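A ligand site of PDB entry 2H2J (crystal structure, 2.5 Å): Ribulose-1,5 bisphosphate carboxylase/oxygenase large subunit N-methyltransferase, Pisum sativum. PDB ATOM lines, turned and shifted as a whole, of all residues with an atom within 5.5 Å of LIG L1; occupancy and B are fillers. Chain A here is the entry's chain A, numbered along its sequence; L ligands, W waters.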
ATOM      1  N   GLU A  32     -25.525  18.087   3.524  1.00  0.00           N
ATOM      2  CA  GLU A  32     -25.836  17.259   2.362  1.00  0.00           C
ATOM      3  C   GLU A  32     -27.068  16.344   2.507  1.00  0.00           C
ATOM      4  O   GLU A  32     -27.165  15.307   1.832  1.00  0.00           O
ATOM      5  CB  GLU A  32     -24.604  16.451   1.959  1.00  0.00           C
ATOM      6  CG  GLU A  32     -23.863  15.766   3.112  1.00  0.00           C
ATOM      7  CD  GLU A  32     -22.762  16.647   3.721  1.00  0.00           C
ATOM      8  OE1 GLU A  32     -21.636  16.669   3.173  1.00  0.00           O
ATOM      9  OE2 GLU A  32     -23.023  17.300   4.759  1.00  0.00           O
ATOM     10  N   GLY A  33     -28.019  16.733   3.356  1.00  0.00           N
ATOM     11  CA  GLY A  33     -29.234  15.941   3.545  1.00  0.00           C
ATOM     12  C   GLY A  33     -29.308  15.245   4.893  1.00  0.00           C
ATOM     13  O   GLY A  33     -29.593  15.866   5.921  1.00  0.00           O
ATOM     14  N   LEU A  34     -29.103  13.938   4.872  1.00  0.00           N
ATOM     15  CA  LEU A  34     -29.085  13.130   6.094  1.00  0.00           C
ATOM     16  C   LEU A  34     -27.784  12.357   5.949  1.00  0.00           C
ATOM     17  O   LEU A  34     -27.368  12.055   4.839  1.00  0.00           O
ATOM     18  CB  LEU A  34     -30.259  12.148   6.143  1.00  0.00           C
ATOM     19  CG  LEU A  34     -31.631  12.680   6.582  1.00  0.00           C
ATOM     20  CD1 LEU A  34     -32.709  11.685   6.171  1.00  0.00           C
ATOM     21  CD2 LEU A  34     -31.639  12.927   8.094  1.00  0.00           C
ATOM     22  N   GLY A  35     -27.129  12.054   7.063  1.00  0.00           N
ATOM     23  CA  GLY A  35     -25.890  11.330   6.928  1.00  0.00           C
ATOM     24  C   GLY A  35     -25.619  10.491   8.139  1.00  0.00           C
ATOM     25  O   GLY A  35     -26.431  10.441   9.060  1.00  0.00           O
ATOM     26  N   ILE A 101     -38.414   8.182   4.823  1.00  0.00           N
ATOM     27  CA  ILE A 101     -37.162   8.906   4.963  1.00  0.00           C
ATOM     28  C   ILE A 101     -36.666   9.410   3.605  1.00  0.00           C
ATOM     29  O   ILE A 101     -36.117  10.508   3.514  1.00  0.00           O
ATOM     30  CB  ILE A 101     -36.077   7.996   5.606  1.00  0.00           C
ATOM     31  CG1 ILE A 101     -36.388   7.823   7.090  1.00  0.00           C
ATOM     32  CG2 ILE A 101     -34.699   8.591   5.421  1.00  0.00           C
ATOM     33  CD1 ILE A 101     -36.582   9.126   7.834  1.00  0.00           C
ATOM     34  N   PRO A 103     -35.928  11.158   0.245  1.00  0.00           N
ATOM     35  CA  PRO A 103     -36.176  12.526  -0.242  1.00  0.00           C
ATOM     36  C   PRO A 103     -37.032  12.416  -1.495  1.00  0.00           C
ATOM     37  O   PRO A 103     -36.798  11.559  -2.356  1.00  0.00           O
ATOM     38  CB  PRO A 103     -34.782  13.045  -0.573  1.00  0.00           C
ATOM     39  CG  PRO A 103     -33.878  12.243   0.328  1.00  0.00           C
ATOM     40  CD  PRO A 103     -34.481  10.857   0.221  1.00  0.00           C
ATOM     41  N   GLU A 105     -37.138  14.501  -3.858  1.00  0.00           N
ATOM     42  CA  GLU A 105     -36.320  14.980  -4.963  1.00  0.00           C
ATOM     43  C   GLU A 105     -34.828  15.148  -4.607  1.00  0.00           C
ATOM     44  O   GLU A 105     -34.449  15.066  -3.427  1.00  0.00           O
ATOM     45  CB  GLU A 105     -36.862  16.348  -5.407  1.00  0.00           C
ATOM     46  CG  GLU A 105     -37.238  16.465  -6.853  1.00  0.00           C
ATOM     47  CD  GLU A 105     -37.924  17.794  -7.154  1.00  0.00           C
ATOM     48  OE1 GLU A 105     -37.318  18.862  -6.912  1.00  0.00           O
ATOM     49  OE2 GLU A 105     -39.077  17.764  -7.635  1.00  0.00           O
ATOM     50  N   THR A 106     -33.998  15.360  -5.616  1.00  0.00           N
ATOM     51  CA  THR A 106     -32.564  15.616  -5.426  1.00  0.00           C
ATOM     52  C   THR A 106     -32.287  16.786  -6.368  1.00  0.00           C
ATOM     53  O   THR A 106     -33.196  17.323  -6.997  1.00  0.00           O
ATOM     54  CB  THR A 106     -31.665  14.448  -5.847  1.00  0.00           C
ATOM     55  OG1 THR A 106     -31.716  14.298  -7.269  1.00  0.00           O
ATOM     56  CG2 THR A 106     -32.099  13.149  -5.179  1.00  0.00           C
ATOM     57  N   ASP A 107     -31.032  17.199  -6.483  1.00  0.00           N
ATOM     58  CA  ASP A 107     -30.729  18.292  -7.373  1.00  0.00           C
ATOM     59  C   ASP A 107     -30.316  17.830  -8.742  1.00  0.00           C
ATOM     60  O   ASP A 107     -29.824  18.620  -9.557  1.00  0.00           O
ATOM     61  CB  ASP A 107     -29.693  19.227  -6.762  1.00  0.00           C
ATOM     62  CG  ASP A 107     -30.318  20.192  -5.789  1.00  0.00           C
ATOM     63  OD1 ASP A 107     -31.480  20.565  -6.023  1.00  0.00           O
ATOM     64  OD2 ASP A 107     -29.659  20.587  -4.797  1.00  0.00           O
ATOM     65  N   SER A 173     -29.076   7.581  -7.780  1.00  0.00           N
ATOM     66  CA  SER A 173     -28.306   8.370  -6.824  1.00  0.00           C
ATOM     67  C   SER A 173     -28.079   7.613  -5.530  1.00  0.00           C
ATOM     68  O   SER A 173     -27.328   8.084  -4.659  1.00  0.00           O
ATOM     69  CB  SER A 173     -29.027   9.697  -6.530  1.00  0.00           C
ATOM     70  OG  SER A 173     -30.221   9.511  -5.789  1.00  0.00           O
ATOM     71  N   ARG A 174     -28.680   6.435  -5.411  1.00  0.00           N
ATOM     72  CA  ARG A 174     -28.560   5.638  -4.193  1.00  0.00           C
ATOM     73  C   ARG A 174     -27.954   4.241  -4.317  1.00  0.00           C
ATOM     74  O   ARG A 174     -27.136   3.851  -3.475  1.00  0.00           O
ATOM     75  CB  ARG A 174     -29.925   5.536  -3.543  1.00  0.00           C
ATOM     76  CG  ARG A 174     -30.385   6.857  -2.981  1.00  0.00           C
ATOM     77  CD  ARG A 174     -31.819   6.815  -2.512  1.00  0.00           C
ATOM     78  NE  ARG A 174     -32.046   7.839  -1.505  1.00  0.00           N
ATOM     79  CZ  ARG A 174     -31.569   7.781  -0.272  1.00  0.00           C
ATOM     80  NH1 ARG A 174     -30.847   6.739   0.106  1.00  0.00           N
ATOM     81  NH2 ARG A 174     -31.820   8.757   0.597  1.00  0.00           N
ATOM     82  N   ASP A 191     -27.644   3.625   2.432  1.00  0.00           N
ATOM     83  CA  ASP A 191     -28.218   4.618   1.544  1.00  0.00           C
ATOM     84  C   ASP A 191     -28.109   6.026   2.131  1.00  0.00           C
ATOM     85  O   ASP A 191     -28.538   6.988   1.513  1.00  0.00           O
ATOM     86  CB  ASP A 191     -29.708   4.308   1.320  1.00  0.00           C
ATOM     87  CG  ASP A 191     -29.999   3.856  -0.093  1.00  0.00           C
ATOM     88  OD1 ASP A 191     -29.499   2.784  -0.509  1.00  0.00           O
ATOM     89  OD2 ASP A 191     -30.745   4.565  -0.798  1.00  0.00           O
ATOM     90  N   LEU A 192     -27.521   6.146   3.315  1.00  0.00           N
ATOM     91  CA  LEU A 192     -27.411   7.444   3.972  1.00  0.00           C
ATOM     92  C   LEU A 192     -26.027   8.075   3.960  1.00  0.00           C
ATOM     93  O   LEU A 192     -25.900   9.283   4.137  1.00  0.00           O
ATOM     94  CB  LEU A 192     -27.905   7.321   5.406  1.00  0.00           C
ATOM     95  CG  LEU A 192     -29.355   6.867   5.507  1.00  0.00           C
ATOM     96  CD1 LEU A 192     -29.718   6.636   6.950  1.00  0.00           C
ATOM     97  CD2 LEU A 192     -30.252   7.939   4.893  1.00  0.00           C
ATOM     98  N   ILE A 193     -24.993   7.264   3.779  1.00  0.00           N
ATOM     99  CA  ILE A 193     -23.637   7.780   3.752  1.00  0.00           C
ATOM    100  C   ILE A 193     -23.406   8.662   2.520  1.00  0.00           C
ATOM    101  O   ILE A 193     -23.681   8.272   1.381  1.00  0.00           O
ATOM    102  CB  ILE A 193     -22.627   6.630   3.767  1.00  0.00           C
ATOM    103  CG1 ILE A 193     -21.207   7.181   3.913  1.00  0.00           C
ATOM    104  CG2 ILE A 193     -22.741   5.840   2.484  1.00  0.00           C
ATOM    105  CD1 ILE A 193     -20.173   6.105   4.104  1.00  0.00           C
ATOM    106  N   ASN A 194     -22.901   9.878   2.762  1.00  0.00           N
ATOM    107  CA  ASN A 194     -22.659  10.823   1.676  1.00  0.00           C
ATOM    108  C   ASN A 194     -21.259  10.741   1.056  1.00  0.00           C
ATOM    109  O   ASN A 194     -20.389   9.958   1.483  1.00  0.00           O
ATOM    110  CB  ASN A 194     -22.920  12.232   2.170  1.00  0.00           C
ATOM    111  CG  ASN A 194     -24.363  12.475   2.467  1.00  0.00           C
ATOM    112  OD1 ASN A 194     -25.206  12.359   1.597  1.00  0.00           O
ATOM    113  ND2 ASN A 194     -24.662  12.817   3.703  1.00  0.00           N
ATOM    114  N   HIS A 195     -21.058  11.565   0.018  1.00  0.00           N
ATOM    115  CA  HIS A 195     -19.798  11.638  -0.715  1.00  0.00           C
ATOM    116  C   HIS A 195     -18.888  12.771  -0.207  1.00  0.00           C
ATOM    117  O   HIS A 195     -19.364  13.816   0.229  1.00  0.00           O
ATOM    118  CB  HIS A 195     -20.099  11.839  -2.204  1.00  0.00           C
ATOM    119  CG  HIS A 195     -18.909  12.184  -3.048  1.00  0.00           C
ATOM    120  ND1 HIS A 195     -18.155  11.230  -3.691  1.00  0.00           N
ATOM    121  CD2 HIS A 195     -18.356  13.384  -3.351  1.00  0.00           C
ATOM    122  CE1 HIS A 195     -17.179  11.822  -4.360  1.00  0.00           C
ATOM    123  NE2 HIS A 195     -17.274  13.130  -4.167  1.00  0.00           N
ATOM    124  N   SER A 196     -17.582  12.531  -0.244  1.00  0.00           N
ATOM    125  CA  SER A 196     -16.613  13.540   0.150  1.00  0.00           C
ATOM    126  C   SER A 196     -15.412  13.445  -0.766  1.00  0.00           C
ATOM    127  O   SER A 196     -15.101  12.362  -1.279  1.00  0.00           O
ATOM    128  CB  SER A 196     -16.143  13.356   1.580  1.00  0.00           C
ATOM    129  OG  SER A 196     -15.040  14.197   1.817  1.00  0.00           O
ATOM    130  N   TYR A 239     -17.858   8.281  -4.190  1.00  0.00           N
ATOM    131  CA  TYR A 239     -18.795   7.663  -5.110  1.00  0.00           C
ATOM    132  C   TYR A 239     -18.127   7.158  -6.385  1.00  0.00           C
ATOM    133  O   TYR A 239     -18.383   6.033  -6.814  1.00  0.00           O
ATOM    134  CB  TYR A 239     -19.924   8.633  -5.452  1.00  0.00           C
ATOM    135  CG  TYR A 239     -20.923   8.845  -4.332  1.00  0.00           C
ATOM    136  CD1 TYR A 239     -22.077   9.599  -4.540  1.00  0.00           C
ATOM    137  CD2 TYR A 239     -20.715   8.298  -3.061  1.00  0.00           C
ATOM    138  CE1 TYR A 239     -23.017   9.802  -3.512  1.00  0.00           C
ATOM    139  CE2 TYR A 239     -21.633   8.493  -2.025  1.00  0.00           C
ATOM    140  CZ  TYR A 239     -22.787   9.248  -2.262  1.00  0.00           C
ATOM    141  OH  TYR A 239     -23.700   9.439  -1.248  1.00  0.00           O
ATOM    142  N   TYR A 252     -26.132  12.313  -9.266  1.00  0.00           N
ATOM    143  CA  TYR A 252     -26.469  12.801  -7.929  1.00  0.00           C
ATOM    144  C   TYR A 252     -26.724  14.270  -8.168  1.00  0.00           C
ATOM    145  O   TYR A 252     -26.613  14.735  -9.303  1.00  0.00           O
ATOM    146  CB  TYR A 252     -25.293  12.606  -6.973  1.00  0.00           C
ATOM    147  CG  TYR A 252     -24.577  11.289  -7.167  1.00  0.00           C
ATOM    148  CD1 TYR A 252     -23.364  11.235  -7.853  1.00  0.00           C
ATOM    149  CD2 TYR A 252     -25.147  10.096  -6.743  1.00  0.00           C
ATOM    150  CE1 TYR A 252     -22.735  10.014  -8.114  1.00  0.00           C
ATOM    151  CE2 TYR A 252     -24.531   8.873  -6.997  1.00  0.00           C
ATOM    152  CZ  TYR A 252     -23.319   8.848  -7.688  1.00  0.00           C
ATOM    153  OH  TYR A 252     -22.706   7.632  -7.963  1.00  0.00           O
ATOM    154  N   GLY A 253     -27.066  15.023  -7.139  1.00  0.00           N
ATOM    155  CA  GLY A 253     -27.320  16.434  -7.396  1.00  0.00           C
ATOM    156  C   GLY A 253     -26.174  17.348  -7.011  1.00  0.00           C
ATOM    157  O   GLY A 253     -26.418  18.415  -6.440  1.00  0.00           O
ATOM    158  N   PHE A 254     -24.933  16.969  -7.321  1.00  0.00           N
ATOM    159  CA  PHE A 254     -23.804  17.828  -6.940  1.00  0.00           C
ATOM    160  C   PHE A 254     -22.591  17.737  -7.863  1.00  0.00           C
ATOM    161  O   PHE A 254     -22.534  16.908  -8.768  1.00  0.00           O
ATOM    162  CB  PHE A 254     -23.374  17.498  -5.500  1.00  0.00           C
ATOM    163  CG  PHE A 254     -22.678  16.156  -5.349  1.00  0.00           C
ATOM    164  CD1 PHE A 254     -21.324  16.033  -5.632  1.00  0.00           C
ATOM    165  CD2 PHE A 254     -23.376  15.036  -4.909  1.00  0.00           C
ATOM    166  CE1 PHE A 254     -20.658  14.808  -5.467  1.00  0.00           C
ATOM    167  CE2 PHE A 254     -22.725  13.797  -4.745  1.00  0.00           C
ATOM    168  CZ  PHE A 254     -21.356  13.688  -5.027  1.00  0.00           C
HETATM  169  N1  LIG L   1     -27.857  11.778   2.506  1.00  0.00           N
HETATM  170  C1  LIG L   1     -28.900  11.622   1.508  1.00  0.00           C
HETATM  171  C2  LIG L   1     -30.309  11.845   2.102  1.00  0.00           C
HETATM  172  O1  LIG L   1     -31.283  11.241   1.600  1.00  0.00           O
HETATM  173  O2  LIG L   1     -30.420  12.609   3.066  1.00  0.00           O
HETATM  174  C3  LIG L   1     -28.842  10.222   0.840  1.00  0.00           C
HETATM  175  C4  LIG L   1     -27.527   9.722   0.233  1.00  0.00           C
HETATM  176  C5  LIG L   1     -27.551   9.276  -1.259  1.00  0.00           C
HETATM  177  N2  LIG L   1     -26.201   8.725  -1.550  1.00  0.00           N
HETATM  178  C6  LIG L   1     -27.683  10.418  -2.318  1.00  0.00           C
HETATM  179  C7  LIG L   1     -27.977  11.859  -1.950  1.00  0.00           C
HETATM  180  O3  LIG L   1     -27.064  12.444  -1.012  1.00  0.00           O
HETATM  181  C8  LIG L   1     -28.045  12.777  -3.180  1.00  0.00           C
HETATM  182  O4  LIG L   1     -29.388  13.212  -3.442  1.00  0.00           O
HETATM  183  C9  LIG L   1     -27.182  13.934  -2.884  1.00  0.00           C
HETATM  184  O5  LIG L   1     -27.987  15.110  -2.992  1.00  0.00           O
HETATM  185  C10 LIG L   1     -26.671  13.751  -1.453  1.00  0.00           C
HETATM  186  N3  LIG L   1     -25.190  13.911  -1.374  1.00  0.00           N
HETATM  187  C11 LIG L   1     -24.209  12.954  -1.240  1.00  0.00           C
HETATM  188  N4  LIG L   1     -22.968  13.367  -1.199  1.00  0.00           N
HETATM  189  C12 LIG L   1     -23.125  14.766  -1.313  1.00  0.00           C
HETATM  190  C13 LIG L   1     -22.200  15.861  -1.360  1.00  0.00           C
HETATM  191  N5  LIG L   1     -20.883  15.685  -1.265  1.00  0.00           N
HETATM  192  N6  LIG L   1     -22.699  17.127  -1.491  1.00  0.00           N
HETATM  193  C14 LIG L   1     -24.046  17.305  -1.593  1.00  0.00           C
HETATM  194  N7  LIG L   1     -25.011  16.369  -1.565  1.00  0.00           N
HETATM  195  C15 LIG L   1     -24.487  15.107  -1.433  1.00  0.00           C
HETATM  196  N1  LG2 L   2     -22.122   3.903  -7.743  1.00  0.00           N
HETATM  197  C1  LG2 L   2     -21.085   4.241  -6.768  1.00  0.00           C
HETATM  198  C2  LG2 L   2     -21.674   5.188  -5.703  1.00  0.00           C
HETATM  199  C3  LG2 L   2     -22.916   4.680  -4.999  1.00  0.00           C
HETATM  200  C4  LG2 L   2     -23.417   5.684  -3.978  1.00  0.00           C
HETATM  201  C5  LG2 L   2     -24.242   5.012  -2.893  1.00  0.00           C
HETATM  202  N2  LG2 L   2     -25.310   5.914  -2.381  1.00  0.00           N
HETATM  203  C6  LG2 L   2     -25.670   5.598  -0.978  1.00  0.00           C
HETATM  204  C7  LG2 L   2     -20.494   2.989  -6.089  1.00  0.00           C
HETATM  205  O1  LG2 L   2     -20.935   1.859  -6.409  1.00  0.00           O
HETATM  206  O2  LG2 L   2     -19.589   3.157  -5.235  1.00  0.00           O
HETATM  207  O   HOH W   1     -28.998  16.659  -4.851  1.00  0.00           O
HETATM  208  O   HOH W   2     -32.834  13.753   2.942  1.00  0.00           O
HETATM  209  O   HOH W   3     -32.976   8.854   3.038  1.00  0.00           O
HETATM  210  O   HOH W   4     -27.825  18.086  -1.999  1.00  0.00           O
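The backbone carbonyl oxygen of His 195 lies within hydrogen-bond range of a nitrogen (N5) of LIG L1 (2.8 Å).
The backbone NH (N) of His 195 sits at hydrogen-bond distance from a nitrogen (N4) of LIG L1 (2.9 Å).
The guanidinium group of Arg 174 lies within salt-bridge range of an oxygen (O1) of LIG L1 (2.7 Å).
O of Arg 174 sits at hydrogen-bond distance from N2 of LG2 L2, at 3.0 Å.
The backbone NH (N) of Leu 34 sits at hydrogen-bond distance from an oxygen (O2) of LIG L1.
O of Leu 34 is in hydrogen-bond range of N1 of LIG L1 (2.4 Å).
The side-chain amide oxygen (OD1) of Asn 194 lies within hydrogen-bond range of a nitrogen (N1) of LIG L1 (2.9 Å).
The backbone carbonyl oxygen (O) of Ser 173 lies close to a nitrogen (N2) of LIG L1 (3.4 Å).
The side-chain hydroxyl (OH) of Tyr 239 is in hydrogen-bond range of a nitrogen (N2) of LIG L1 (2.6 Å).
N2 of LG2 L2 lies close to N2 of LIG L1 (3.1 Å).
Water W1 lies within hydrogen-bond range of O5 of LIG L1 (2.6 Å), N of Asp 107 (2.7 Å) and N of Gly 253 (3.4 Å).
Water W3 bridges NH2 of Arg 174 and O1 of LIG L1.
Merely in contact with LIG L1: Pro 103, Asp 191, Thr 106, Gly 33, Glu 32, Leu 192, Phe 254 and Ile 193.
Of the 21 residues printed, 14 come within 4 Å of LIG L1.
Along chain A the residues within 4 Å of LIG L1 span positions 32 to 254.
The side-chain hydroxyl of Tyr 239 is in hydrogen-bond range of the backbone carbonyl oxygen of Ile 193 (2.9 Å).
The guanidinium group (NE) of Arg 174 lies within salt-bridge range of the side-chain carboxylate (OD2) of Asp 191.
N of Tyr 239 sits at hydrogen-bond distance from ND1 of His 195, 3.0 Å away.
The backbone carbonyl oxygen (O) of Leu 34 lies within hydrogen-bond range of the side-chain amide nitrogen (ND2) of Asn 194 (3.0 Å).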
